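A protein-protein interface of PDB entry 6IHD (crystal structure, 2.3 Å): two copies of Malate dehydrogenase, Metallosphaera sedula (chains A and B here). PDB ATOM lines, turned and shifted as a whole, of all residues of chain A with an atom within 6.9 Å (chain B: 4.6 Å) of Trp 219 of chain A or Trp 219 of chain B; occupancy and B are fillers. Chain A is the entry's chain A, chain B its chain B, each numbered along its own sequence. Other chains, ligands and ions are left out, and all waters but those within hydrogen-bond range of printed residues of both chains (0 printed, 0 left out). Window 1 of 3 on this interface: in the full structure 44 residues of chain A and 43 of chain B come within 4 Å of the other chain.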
ATOM      1  N   GLY A   9      29.456 -17.740  -3.993  1.00  0.00           N
ATOM      2  CA  GLY A   9      28.485 -16.859  -3.321  1.00  0.00           C
ATOM      3  C   GLY A   9      28.237 -15.576  -4.116  1.00  0.00           C
ATOM      4  O   GLY A   9      28.630 -15.457  -5.271  1.00  0.00           O
ATOM      5  N   LYS A  10      27.636 -14.597  -3.460  1.00  0.00           N
ATOM      6  CA  LYS A  10      27.309 -13.307  -4.057  1.00  0.00           C
ATOM      7  C   LYS A  10      28.354 -12.737  -5.034  1.00  0.00           C
ATOM      8  O   LYS A  10      28.047 -12.582  -6.215  1.00  0.00           O
ATOM      9  CB  LYS A  10      27.043 -12.300  -2.940  1.00  0.00           C
ATOM     10  CG  LYS A  10      25.643 -12.495  -2.290  1.00  0.00           C
ATOM     11  CD  LYS A  10      25.471 -11.685  -0.998  1.00  0.00           C
ATOM     12  CE  LYS A  10      26.595 -11.947   0.023  1.00  0.00           C
ATOM     13  NZ  LYS A  10      26.165 -12.202   1.430  1.00  0.00           N
ATOM     14  N   ILE A  11      29.565 -12.398  -4.558  1.00  0.00           N
ATOM     15  CA  ILE A  11      30.583 -11.853  -5.459  1.00  0.00           C
ATOM     16  C   ILE A  11      31.080 -12.887  -6.496  1.00  0.00           C
ATOM     17  O   ILE A  11      31.280 -12.519  -7.648  1.00  0.00           O
ATOM     18  CB  ILE A  11      31.770 -11.189  -4.722  1.00  0.00           C
ATOM     19  CG1 ILE A  11      32.476 -10.185  -5.625  1.00  0.00           C
ATOM     20  CG2 ILE A  11      32.809 -12.178  -4.226  1.00  0.00           C
ATOM     21  CD1 ILE A  11      31.551  -9.105  -6.164  1.00  0.00           C
ATOM     22  N   GLY A  12      31.249 -14.166  -6.115  1.00  0.00           N
ATOM     23  CA  GLY A  12      31.665 -15.179  -7.103  1.00  0.00           C
ATOM     24  C   GLY A  12      30.666 -15.427  -8.235  1.00  0.00           C
ATOM     25  O   GLY A  12      31.030 -15.503  -9.397  1.00  0.00           O
ATOM     26  N   GLN A  13      29.398 -15.576  -7.887  1.00  0.00           N
ATOM     27  CA  GLN A  13      28.334 -15.650  -8.917  1.00  0.00           C
ATOM     28  C   GLN A  13      28.284 -14.433  -9.870  1.00  0.00           C
ATOM     29  O   GLN A  13      28.195 -14.591 -11.076  1.00  0.00           O
ATOM     30  CB  GLN A  13      26.988 -15.795  -8.252  1.00  0.00           C
ATOM     31  CG  GLN A  13      26.768 -17.172  -7.690  1.00  0.00           C
ATOM     32  CD  GLN A  13      25.444 -17.244  -6.956  1.00  0.00           C
ATOM     33  OE1 GLN A  13      24.448 -16.722  -7.418  1.00  0.00           O
ATOM     34  NE2 GLN A  13      25.441 -17.847  -5.802  1.00  0.00           N
ATOM     35  N   THR A  14      28.374 -13.226  -9.320  1.00  0.00           N
ATOM     36  CA  THR A  14      28.356 -12.045 -10.129  1.00  0.00           C
ATOM     37  C   THR A  14      29.496 -12.003 -11.098  1.00  0.00           C
ATOM     38  O   THR A  14      29.297 -11.789 -12.306  1.00  0.00           O
ATOM     39  CB  THR A  14      28.399 -10.790  -9.283  1.00  0.00           C
ATOM     40  OG1 THR A  14      27.456 -10.933  -8.232  1.00  0.00           O
ATOM     41  CG2 THR A  14      28.013  -9.600 -10.117  1.00  0.00           C
ATOM     42  N   ILE A  15      30.697 -12.212 -10.599  1.00  0.00           N
ATOM     43  CA  ILE A  15      31.852 -12.167 -11.497  1.00  0.00           C
ATOM     44  C   ILE A  15      31.689 -13.248 -12.542  1.00  0.00           C
ATOM     45  O   ILE A  15      31.990 -12.996 -13.705  1.00  0.00           O
ATOM     46  CB  ILE A  15      33.163 -12.425 -10.777  1.00  0.00           C
ATOM     47  CG1 ILE A  15      33.427 -11.292  -9.762  1.00  0.00           C
ATOM     48  CG2 ILE A  15      34.297 -12.471 -11.793  1.00  0.00           C
ATOM     49  CD1 ILE A  15      34.385 -11.684  -8.648  1.00  0.00           C
ATOM     50  N   TYR A  17      28.944 -14.701 -13.762  1.00  0.00           N
ATOM     51  CA  TYR A  17      27.889 -14.250 -14.680  1.00  0.00           C
ATOM     52  C   TYR A  17      28.395 -13.244 -15.736  1.00  0.00           C
ATOM     53  O   TYR A  17      28.313 -13.492 -16.910  1.00  0.00           O
ATOM     54  CB  TYR A  17      26.691 -13.670 -13.884  1.00  0.00           C
ATOM     55  CG  TYR A  17      25.586 -13.152 -14.765  1.00  0.00           C
ATOM     56  CD1 TYR A  17      24.699 -14.009 -15.346  1.00  0.00           C
ATOM     57  CD2 TYR A  17      25.466 -11.794 -15.040  1.00  0.00           C
ATOM     58  CE1 TYR A  17      23.718 -13.545 -16.192  1.00  0.00           C
ATOM     59  CE2 TYR A  17      24.484 -11.307 -15.885  1.00  0.00           C
ATOM     60  CZ  TYR A  17      23.600 -12.179 -16.453  1.00  0.00           C
ATOM     61  OH  TYR A  17      22.596 -11.731 -17.280  1.00  0.00           O
ATOM     62  N   SER A  18      28.955 -12.147 -15.259  1.00  0.00           N
ATOM     63  CA  SER A  18      29.470 -11.037 -16.044  1.00  0.00           C
ATOM     64  C   SER A  18      30.603 -11.434 -17.003  1.00  0.00           C
ATOM     65  O   SER A  18      30.677 -10.946 -18.129  1.00  0.00           O
ATOM     66  CB  SER A  18      29.941  -9.950 -15.050  1.00  0.00           C
ATOM     67  OG  SER A  18      30.410  -8.774 -15.673  1.00  0.00           O
ATOM     68  N   PHE A  41      23.483 -23.026  -9.504  1.00  0.00           N
ATOM     69  CA  PHE A  41      24.057 -21.900 -10.207  1.00  0.00           C
ATOM     70  C   PHE A  41      24.356 -22.244 -11.657  1.00  0.00           C
ATOM     71  O   PHE A  41      24.042 -21.467 -12.517  1.00  0.00           O
ATOM     72  CB  PHE A  41      25.342 -21.423  -9.541  1.00  0.00           C
ATOM     73  CG  PHE A  41      25.975 -20.229 -10.223  1.00  0.00           C
ATOM     74  CD1 PHE A  41      25.214 -19.083 -10.517  1.00  0.00           C
ATOM     75  CD2 PHE A  41      27.353 -20.209 -10.509  1.00  0.00           C
ATOM     76  CE1 PHE A  41      25.801 -17.968 -11.083  1.00  0.00           C
ATOM     77  CE2 PHE A  41      27.945 -19.104 -11.109  1.00  0.00           C
ATOM     78  CZ  PHE A  41      27.165 -18.005 -11.434  1.00  0.00           C
ATOM     79  N   GLU A  44      21.123 -22.082 -13.602  1.00  0.00           N
ATOM     80  CA  GLU A  44      20.769 -20.671 -13.817  1.00  0.00           C
ATOM     81  C   GLU A  44      21.553 -20.063 -14.966  1.00  0.00           C
ATOM     82  O   GLU A  44      20.978 -19.317 -15.742  1.00  0.00           O
ATOM     83  CB  GLU A  44      21.084 -19.856 -12.550  1.00  0.00           C
ATOM     84  CG  GLU A  44      20.110 -20.080 -11.424  1.00  0.00           C
ATOM     85  CD  GLU A  44      19.052 -18.995 -11.445  1.00  0.00           C
ATOM     86  OE1 GLU A  44      18.309 -18.902 -12.480  1.00  0.00           O
ATOM     87  OE2 GLU A  44      19.012 -18.212 -10.463  1.00  0.00           O
ATOM     88  N   LEU A  45      22.863 -20.375 -15.059  1.00  0.00           N
ATOM     89  CA  LEU A  45      23.712 -19.918 -16.174  1.00  0.00           C
ATOM     90  C   LEU A  45      23.233 -20.462 -17.477  1.00  0.00           C
ATOM     91  O   LEU A  45      23.121 -19.693 -18.403  1.00  0.00           O
ATOM     92  CB  LEU A  45      25.199 -20.252 -15.999  1.00  0.00           C
ATOM     93  CG  LEU A  45      25.866 -19.510 -14.798  1.00  0.00           C
ATOM     94  CD1 LEU A  45      27.253 -20.053 -14.485  1.00  0.00           C
ATOM     95  CD2 LEU A  45      25.929 -18.020 -15.049  1.00  0.00           C
ATOM     96  N   HIS A  47      20.238 -21.425 -18.366  1.00  0.00           N
ATOM     97  CA  HIS A  47      19.008 -20.798 -18.789  1.00  0.00           C
ATOM     98  C   HIS A  47      19.246 -19.384 -19.355  1.00  0.00           C
ATOM     99  O   HIS A  47      18.676 -19.008 -20.396  1.00  0.00           O
ATOM    100  CB  HIS A  47      17.989 -20.730 -17.641  1.00  0.00           C
ATOM    101  CG  HIS A  47      17.766 -22.022 -16.968  1.00  0.00           C
ATOM    102  ND1 HIS A  47      17.353 -22.108 -15.668  1.00  0.00           N
ATOM    103  CD2 HIS A  47      17.944 -23.290 -17.396  1.00  0.00           C
ATOM    104  CE1 HIS A  47      17.266 -23.374 -15.316  1.00  0.00           C
ATOM    105  NE2 HIS A  47      17.636 -24.112 -16.347  1.00  0.00           N
ATOM    106  N   ALA A  48      20.069 -18.605 -18.669  1.00  0.00           N
ATOM    107  CA  ALA A  48      20.527 -17.340 -19.214  1.00  0.00           C
ATOM    108  C   ALA A  48      21.240 -17.505 -20.560  1.00  0.00           C
ATOM    109  O   ALA A  48      20.994 -16.741 -21.489  1.00  0.00           O
ATOM    110  CB  ALA A  48      21.458 -16.632 -18.256  1.00  0.00           C
ATOM    111  N   ILE A 214      22.025  -3.141   1.971  1.00  0.00           N
ATOM    112  CA  ILE A 214      21.709  -4.238   1.074  1.00  0.00           C
ATOM    113  C   ILE A 214      21.933  -5.673   1.579  1.00  0.00           C
ATOM    114  O   ILE A 214      21.022  -6.446   1.522  1.00  0.00           O
ATOM    115  CB  ILE A 214      22.284  -3.995  -0.330  1.00  0.00           C
ATOM    116  CG1 ILE A 214      21.755  -2.685  -0.870  1.00  0.00           C
ATOM    117  CG2 ILE A 214      21.861  -5.078  -1.282  1.00  0.00           C
ATOM    118  CD1 ILE A 214      22.119  -2.419  -2.301  1.00  0.00           C
ATOM    119  N   GLY A 216      26.304  -7.170   1.148  1.00  0.00           N
ATOM    120  CA  GLY A 216      27.115  -6.142   0.591  1.00  0.00           C
ATOM    121  C   GLY A 216      26.991  -5.906  -0.865  1.00  0.00           C
ATOM    122  O   GLY A 216      25.925  -5.804  -1.376  1.00  0.00           O
ATOM    123  N   THR A 217      28.145  -5.770  -1.476  1.00  0.00           N
ATOM    124  CA  THR A 217      28.329  -5.269  -2.763  1.00  0.00           C
ATOM    125  C   THR A 217      28.452  -6.431  -3.734  1.00  0.00           C
ATOM    126  O   THR A 217      29.187  -7.373  -3.460  1.00  0.00           O
ATOM    127  CB  THR A 217      29.652  -4.498  -2.793  1.00  0.00           C
ATOM    128  OG1 THR A 217      30.721  -5.402  -2.489  1.00  0.00           O
ATOM    129  CG2 THR A 217      29.647  -3.360  -1.773  1.00  0.00           C
ATOM    130  N   THR A 218      27.770  -6.346  -4.879  1.00  0.00           N
ATOM    131  CA  THR A 218      27.833  -7.384  -5.913  1.00  0.00           C
ATOM    132  C   THR A 218      28.063  -6.762  -7.266  1.00  0.00           C
ATOM    133  O   THR A 218      29.158  -6.832  -7.808  1.00  0.00           O
ATOM    134  CB  THR A 218      26.539  -8.200  -5.884  1.00  0.00           C
ATOM    135  OG1 THR A 218      25.427  -7.355  -6.225  1.00  0.00           O
ATOM    136  CG2 THR A 218      26.304  -8.743  -4.497  1.00  0.00           C
ATOM    137  N   TRP A 219      27.048  -6.051  -7.767  1.00  0.00           N
ATOM    138  CA  TRP A 219      27.019  -5.529  -9.147  1.00  0.00           C
ATOM    139  C   TRP A 219      28.296  -4.744  -9.567  1.00  0.00           C
ATOM    140  O   TRP A 219      28.832  -4.928 -10.668  1.00  0.00           O
ATOM    141  CB  TRP A 219      25.746  -4.654  -9.345  1.00  0.00           C
ATOM    142  CG  TRP A 219      24.480  -5.383  -8.943  1.00  0.00           C
ATOM    143  CD1 TRP A 219      23.707  -5.153  -7.837  1.00  0.00           C
ATOM    144  CD2 TRP A 219      23.933  -6.528  -9.579  1.00  0.00           C
ATOM    145  NE1 TRP A 219      22.674  -6.066  -7.764  1.00  0.00           N
ATOM    146  CE2 TRP A 219      22.788  -6.923  -8.830  1.00  0.00           C
ATOM    147  CE3 TRP A 219      24.298  -7.274 -10.698  1.00  0.00           C
ATOM    148  CZ2 TRP A 219      22.011  -8.034  -9.182  1.00  0.00           C
ATOM    149  CZ3 TRP A 219      23.503  -8.376 -11.069  1.00  0.00           C
ATOM    150  CH2 TRP A 219      22.377  -8.739 -10.311  1.00  0.00           C
ATOM    151  N   GLY A 220      28.731  -3.839  -8.691  1.00  0.00           N
ATOM    152  CA  GLY A 220      29.822  -2.934  -8.967  1.00  0.00           C
ATOM    153  C   GLY A 220      31.112  -3.725  -9.092  1.00  0.00           C
ATOM    154  O   GLY A 220      31.647  -3.859 -10.196  1.00  0.00           O
ATOM    155  N   PRO A 221      31.596  -4.298  -7.986  1.00  0.00           N
ATOM    156  CA  PRO A 221      32.864  -5.073  -8.047  1.00  0.00           C
ATOM    157  C   PRO A 221      32.798  -6.357  -8.888  1.00  0.00           C
ATOM    158  O   PRO A 221      33.797  -6.740  -9.541  1.00  0.00           O
ATOM    159  CB  PRO A 221      33.187  -5.380  -6.591  1.00  0.00           C
ATOM    160  CG  PRO A 221      31.990  -5.041  -5.806  1.00  0.00           C
ATOM    161  CD  PRO A 221      31.114  -4.117  -6.611  1.00  0.00           C
ATOM    162  N   GLY A 222      31.643  -7.001  -8.915  1.00  0.00           N
ATOM    163  CA  GLY A 222      31.452  -8.088  -9.886  1.00  0.00           C
ATOM    164  C   GLY A 222      31.791  -7.696 -11.325  1.00  0.00           C
ATOM    165  O   GLY A 222      32.563  -8.371 -11.992  1.00  0.00           O
ATOM    166  N   THR A 223      31.261  -6.566 -11.783  1.00  0.00           N
ATOM    167  CA  THR A 223      31.414  -6.153 -13.169  1.00  0.00           C
ATOM    168  C   THR A 223      32.865  -5.719 -13.351  1.00  0.00           C
ATOM    169  O   THR A 223      33.511  -6.026 -14.347  1.00  0.00           O
ATOM    170  CB  THR A 223      30.441  -5.001 -13.499  1.00  0.00           C
ATOM    171  OG1 THR A 223      29.083  -5.392 -13.226  1.00  0.00           O
ATOM    172  CG2 THR A 223      30.572  -4.546 -14.932  1.00  0.00           C
ATOM    173  N   ILE A 224      33.393  -5.033 -12.356  1.00  0.00           N
ATOM    174  CA  ILE A 224      34.731  -4.420 -12.472  1.00  0.00           C
ATOM    175  C   ILE A 224      35.849  -5.484 -12.551  1.00  0.00           C
ATOM    176  O   ILE A 224      36.787  -5.385 -13.343  1.00  0.00           O
ATOM    177  CB  ILE A 224      34.932  -3.456 -11.285  1.00  0.00           C
ATOM    178  CG1 ILE A 224      34.090  -2.194 -11.536  1.00  0.00           C
ATOM    179  CG2 ILE A 224      36.409  -3.113 -11.132  1.00  0.00           C
ATOM    180  CD1 ILE A 224      33.819  -1.287 -10.345  1.00  0.00           C
ATOM    181  N   GLN B  13      16.674  -6.148  -9.483  1.00  0.00           N
ATOM    182  CA  GLN B  13      18.047  -5.722  -9.716  1.00  0.00           C
ATOM    183  C   GLN B  13      18.721  -6.485 -10.853  1.00  0.00           C
ATOM    184  O   GLN B  13      19.377  -5.888 -11.660  1.00  0.00           O
ATOM    185  CB  GLN B  13      18.867  -5.920  -8.459  1.00  0.00           C
ATOM    186  CG  GLN B  13      18.607  -4.904  -7.355  1.00  0.00           C
ATOM    187  CD  GLN B  13      19.332  -5.267  -6.070  1.00  0.00           C
ATOM    188  OE1 GLN B  13      20.532  -5.584  -6.072  1.00  0.00           O
ATOM    189  NE2 GLN B  13      18.604  -5.255  -4.979  1.00  0.00           N
ATOM    190  N   THR B  14      18.573  -7.798 -10.897  1.00  0.00           N
ATOM    191  CA  THR B  14      19.181  -8.584 -11.952  1.00  0.00           C
ATOM    192  C   THR B  14      18.619  -8.108 -13.268  1.00  0.00           C
ATOM    193  O   THR B  14      19.390  -7.854 -14.181  1.00  0.00           O
ATOM    194  CB  THR B  14      18.903 -10.078 -11.752  1.00  0.00           C
ATOM    195  OG1 THR B  14      19.135 -10.371 -10.386  1.00  0.00           O
ATOM    196  CG2 THR B  14      19.804 -10.934 -12.595  1.00  0.00           C
ATOM    197  N   TYR B  17      20.050  -4.673 -14.074  1.00  0.00           N
ATOM    198  CA  TYR B  17      21.487  -4.734 -14.383  1.00  0.00           C
ATOM    199  C   TYR B  17      21.658  -5.173 -15.768  1.00  0.00           C
ATOM    200  O   TYR B  17      22.417  -4.582 -16.528  1.00  0.00           O
ATOM    201  CB  TYR B  17      22.192  -5.734 -13.480  1.00  0.00           C
ATOM    202  CG  TYR B  17      23.646  -5.963 -13.828  1.00  0.00           C
ATOM    203  CD1 TYR B  17      24.621  -5.049 -13.459  1.00  0.00           C
ATOM    204  CD2 TYR B  17      24.054  -7.117 -14.493  1.00  0.00           C
ATOM    205  CE1 TYR B  17      25.950  -5.262 -13.775  1.00  0.00           C
ATOM    206  CE2 TYR B  17      25.379  -7.350 -14.788  1.00  0.00           C
ATOM    207  CZ  TYR B  17      26.328  -6.418 -14.429  1.00  0.00           C
ATOM    208  OH  TYR B  17      27.653  -6.629 -14.736  1.00  0.00           O
ATOM    209  N   PHE B  41      21.625   0.711  -4.590  1.00  0.00           N
ATOM    210  CA  PHE B  41      21.674   0.028  -5.881  1.00  0.00           C
ATOM    211  C   PHE B  41      22.131   0.938  -7.019  1.00  0.00           C
ATOM    212  O   PHE B  41      22.929   0.510  -7.888  1.00  0.00           O
ATOM    213  CB  PHE B  41      20.321  -0.642  -6.203  1.00  0.00           C
ATOM    214  CG  PHE B  41      20.286  -1.348  -7.527  1.00  0.00           C
ATOM    215  CD1 PHE B  41      21.267  -2.244  -7.869  1.00  0.00           C
ATOM    216  CD2 PHE B  41      19.205  -1.157  -8.411  1.00  0.00           C
ATOM    217  CE1 PHE B  41      21.210  -2.898  -9.076  1.00  0.00           C
ATOM    218  CE2 PHE B  41      19.141  -1.811  -9.607  1.00  0.00           C
ATOM    219  CZ  PHE B  41      20.156  -2.670  -9.947  1.00  0.00           C
ATOM    220  N   GLU B  44      25.922   1.255  -6.876  1.00  0.00           N
ATOM    221  CA  GLU B  44      26.432   0.005  -7.476  1.00  0.00           C
ATOM    222  C   GLU B  44      26.441   0.039  -9.000  1.00  0.00           C
ATOM    223  O   GLU B  44      27.478  -0.212  -9.650  1.00  0.00           O
ATOM    224  CB  GLU B  44      25.619  -1.204  -7.025  1.00  0.00           C
ATOM    225  CG  GLU B  44      25.926  -1.675  -5.628  1.00  0.00           C
ATOM    226  CD  GLU B  44      26.961  -2.782  -5.570  1.00  0.00           C
ATOM    227  OE1 GLU B  44      28.147  -2.573  -5.938  1.00  0.00           O
ATOM    228  OE2 GLU B  44      26.561  -3.862  -5.104  1.00  0.00           O
ATOM    229  N   ALA B  48      29.656   0.025 -11.708  1.00  0.00           N
ATOM    230  CA  ALA B  48      29.699  -0.920 -12.827  1.00  0.00           C
ATOM    231  C   ALA B  48      29.804  -0.201 -14.148  1.00  0.00           C
ATOM    232  O   ALA B  48      30.596  -0.599 -15.026  1.00  0.00           O
ATOM    233  CB  ALA B  48      28.476  -1.805 -12.795  1.00  0.00           C
ATOM    234  N   THR B 217      15.536 -17.418  -7.526  1.00  0.00           N
ATOM    235  CA  THR B 217      15.884 -17.576  -8.938  1.00  0.00           C
ATOM    236  C   THR B 217      16.199 -16.185  -9.436  1.00  0.00           C
ATOM    237  O   THR B 217      15.448 -15.236  -9.159  1.00  0.00           O
ATOM    238  CB  THR B 217      14.740 -18.318  -9.631  1.00  0.00           C
ATOM    239  OG1 THR B 217      15.241 -18.956 -10.799  1.00  0.00           O
ATOM    240  CG2 THR B 217      13.629 -17.431  -9.962  1.00  0.00           C
ATOM    241  N   THR B 218      17.384 -15.997 -10.005  1.00  0.00           N
ATOM    242  CA  THR B 218      17.830 -14.685 -10.418  1.00  0.00           C
ATOM    243  C   THR B 218      18.499 -14.649 -11.785  1.00  0.00           C
ATOM    244  O   THR B 218      17.917 -14.127 -12.703  1.00  0.00           O
ATOM    245  CB  THR B 218      18.707 -14.013  -9.392  1.00  0.00           C
ATOM    246  OG1 THR B 218      19.954 -14.714  -9.280  1.00  0.00           O
ATOM    247  CG2 THR B 218      17.952 -13.903  -8.043  1.00  0.00           C
ATOM    248  N   TRP B 219      19.685 -15.202 -11.944  1.00  0.00           N
ATOM    249  CA  TRP B 219      20.452 -14.987 -13.192  1.00  0.00           C
ATOM    250  C   TRP B 219      19.645 -15.379 -14.466  1.00  0.00           C
ATOM    251  O   TRP B 219      19.577 -14.641 -15.448  1.00  0.00           O
ATOM    252  CB  TRP B 219      21.777 -15.738 -13.139  1.00  0.00           C
ATOM    253  CG  TRP B 219      22.484 -15.444 -11.857  1.00  0.00           C
ATOM    254  CD1 TRP B 219      22.536 -16.230 -10.735  1.00  0.00           C
ATOM    255  CD2 TRP B 219      23.162 -14.224 -11.539  1.00  0.00           C
ATOM    256  NE1 TRP B 219      23.239 -15.561  -9.732  1.00  0.00           N
ATOM    257  CE2 TRP B 219      23.647 -14.345 -10.207  1.00  0.00           C
ATOM    258  CE3 TRP B 219      23.368 -13.019 -12.237  1.00  0.00           C
ATOM    259  CZ2 TRP B 219      24.364 -13.319  -9.563  1.00  0.00           C
ATOM    260  CZ3 TRP B 219      24.106 -12.025 -11.632  1.00  0.00           C
ATOM    261  CH2 TRP B 219      24.592 -12.177 -10.277  1.00  0.00           C
ATOM    262  N   GLY B 220      18.990 -16.504 -14.385  1.00  0.00           N
ATOM    263  CA  GLY B 220      18.217 -17.030 -15.485  1.00  0.00           C
ATOM    264  C   GLY B 220      17.084 -16.119 -15.841  1.00  0.00           C
ATOM    265  O   GLY B 220      17.112 -15.538 -16.904  1.00  0.00           O
ATOM    266  N   PRO B 221      16.114 -15.946 -14.930  1.00  0.00           N
ATOM    267  CA  PRO B 221      14.935 -15.138 -15.301  1.00  0.00           C
ATOM    268  C   PRO B 221      15.283 -13.703 -15.609  1.00  0.00           C
ATOM    269  O   PRO B 221      14.696 -13.111 -16.498  1.00  0.00           O
ATOM    270  CB  PRO B 221      14.020 -15.242 -14.074  1.00  0.00           C
ATOM    271  CG  PRO B 221      14.401 -16.525 -13.460  1.00  0.00           C
ATOM    272  CD  PRO B 221      15.895 -16.644 -13.649  1.00  0.00           C
ATOM    273  N   GLY B 222      16.264 -13.176 -14.901  1.00  0.00           N
ATOM    274  CA  GLY B 222      16.638 -11.785 -15.024  1.00  0.00           C
ATOM    275  C   GLY B 222      17.294 -11.464 -16.353  1.00  0.00           C
ATOM    276  O   GLY B 222      17.015 -10.438 -16.922  1.00  0.00           O
ATOM    277  N   THR B 223      18.135 -12.354 -16.869  1.00  0.00           N
ATOM    278  CA  THR B 223      18.664 -12.171 -18.219  1.00  0.00           C
ATOM    279  C   THR B 223      17.531 -12.403 -19.245  1.00  0.00           C
ATOM    280  O   THR B 223      17.378 -11.673 -20.219  1.00  0.00           O
ATOM    281  CB  THR B 223      19.778 -13.196 -18.530  1.00  0.00           C
ATOM    282  OG1 THR B 223      20.740 -13.196 -17.503  1.00  0.00           O
ATOM    283  CG2 THR B 223      20.465 -12.888 -19.860  1.00  0.00           C
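Tyr 17 of chain A touches Trp 219 of chain B, and with the chains exchanged Trp 219 of chain A touches Tyr 17 of chain B. Tyr 17 of chain A touches Thr 223 of chain B, and with the chains exchanged Thr 223 of chain A touches Tyr 17 of chain B. Glu 44 of chain A touches Gly 220 of chain B, and with the chains exchanged Gly 220 of chain A touches Glu 44 of chain B. Ala 48 of chain A touches Thr 223 of chain B, and with the chains exchanged Thr 223 of chain A touches Ala 48 of chain B. 13 positions are printed for both chains.
The side-chain hydroxyl (OG1) of Thr 14 of chain A lies within hydrogen-bond range of the backbone carbonyl oxygen (O) of Lys 10 of chain A (2.7 Å). The indole nitrogen (NE1) of Trp 219 of chain A sits close to the side-chain hydroxyl (OG1) of Thr 218 of chain A. The backbone carbonyl oxygen (O) of Trp 219 of chain A is in hydrogen-bond range of the side-chain hydroxyl (OG1) of Thr 223 of chain A. The side-chain hydroxyl of Thr 218 of chain B sits close to the indole nitrogen of Trp 219 of chain B, at 3.4 Å. The backbone carbonyl oxygen (O) of Trp 219 of chain B is in hydrogen-bond range of the side-chain hydroxyl (OG1) of Thr 223 of chain B (2.8 Å).
Tyr 17 of chain A touches Trp 219 of chain B (CG to CE3, 3.4 Å). Tyr 17 of chain B touches Ser 18 of chain A. Phe 41 of chain A touches Trp 219 of chain B. Trp 219 of chain B touches Ala 48 of chain A (O to CB, 3.9 Å). CA of Thr 217 of chain A touches OE2 of Glu 44 of chain B, at 3.3 Å. Thr 14 of chain B touches Trp 219 of chain A. Trp 219 of chain A touches Tyr 17 of chain B (CE3 to CG, 3.5 Å). Phe 41 of chain B touches Trp 219 of chain A (CE1 to CD1, 3.6 Å). Ala 48 of chain B touches Trp 219 of chain A. Trp 219 of chain B touches Trp 219 of chain A.
Trp 219 of chain A touches just these residues of chain B: Gln 13 (2.8 Å), Thr 14 (3.6 Å), Tyr 17 (3.5 Å), Phe 41 (3.6 Å), Glu 44 (3.5 Å), Ala 48 (3.8 Å) and Trp 219 (3.7 Å). Trp 219 of chain B touches just these residues of chain A: Gln 13 (2.9 Å), Thr 14 (3.7 Å), Tyr 17 (3.4 Å), Phe 41 (3.7 Å), Glu 44 (3.4 Å), Ala 48 (3.9 Å) and Trp 219 (3.7 Å). Printed residues of chain B within 4 Å of Phe 41 of chain A: Trp 219. Of the printed residues of chain B, Pro 221 of chain A touches Glu 44. Of the printed residues of chain B, Thr 14 of chain A touches Trp 219. Printed residues of chain B within 4 Å of Thr 223 of chain A: Tyr 17 and Ala 48. Printed residues of chain B within 4 Å of Thr 217 of chain A: Glu 44 (3.3 Å). The nearest printed residue of chain B that does not touch Trp 219 of chain A is Thr 218 of chain B (6.5 Å).
The side-chain amide oxygen of Gln 13 of chain A is in hydrogen-bond range of the indole nitrogen of Trp 219 of chain B (2.9 Å). The side-chain hydroxyl (OG1) of Thr 217 of chain B lies within hydrogen-bond range of the side-chain carboxylate (OE1) of Glu 44 of chain A, at 3.5 Å. The side-chain carboxylate of Glu 44 of chain A lies within hydrogen-bond range of the backbone NH of Thr 218 of chain B, at 2.8 Å. The side-chain carboxylate (OE2) of Glu 44 of chain A is in hydrogen-bond range of the backbone NH (N) of Trp 219 of chain B (3.4 Å). The backbone NH of Gly 220 of chain B sits at hydrogen-bond distance from the side-chain carboxylate of Glu 44 of chain A, at 3.1 Å. N of Thr 218 of chain A lies within hydrogen-bond range of OE2 of Glu 44 of chain B (2.8 Å). OE1 of Gln 13 of chain B lies within hydrogen-bond range of NE1 of Trp 219 of chain A, at 2.8 Å. N of Trp 219 of chain A is in hydrogen-bond range of OE2 of Glu 44 of chain B (3.5 Å). OE1 of Glu 44 of chain B is in hydrogen-bond range of N of Gly 220 of chain A (3.1 Å). OG1 of Thr 223 of chain A lies within hydrogen-bond range of OH of Tyr 17 of chain B (2.4 Å). OH of Tyr 17 of chain A sits close to OG1 of Thr 223 of chain B, at 2.4 Å.
Of the 24 printed residues of chain A, 14 touch a printed residue of chain B. Printed residues of chain A that touch a printed residue of chain B: Gln 13, Thr 14, Tyr 17, Ser 18, Phe 41, Glu 44, Ala 48, Ile 214, Thr 217, Thr 218, Trp 219, Gly 220, Pro 221 and Thr 223. Hydrophobic or aromatic side chains of chain B that line the printed part of chain A: Tyr 17, Phe 41, Ala 48, Trp 219 and Pro 221. Among the printed residues, no Asp or Glu carboxylate lies within 4 Å of a Lys or Arg side-chain nitrogen of the other chain.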
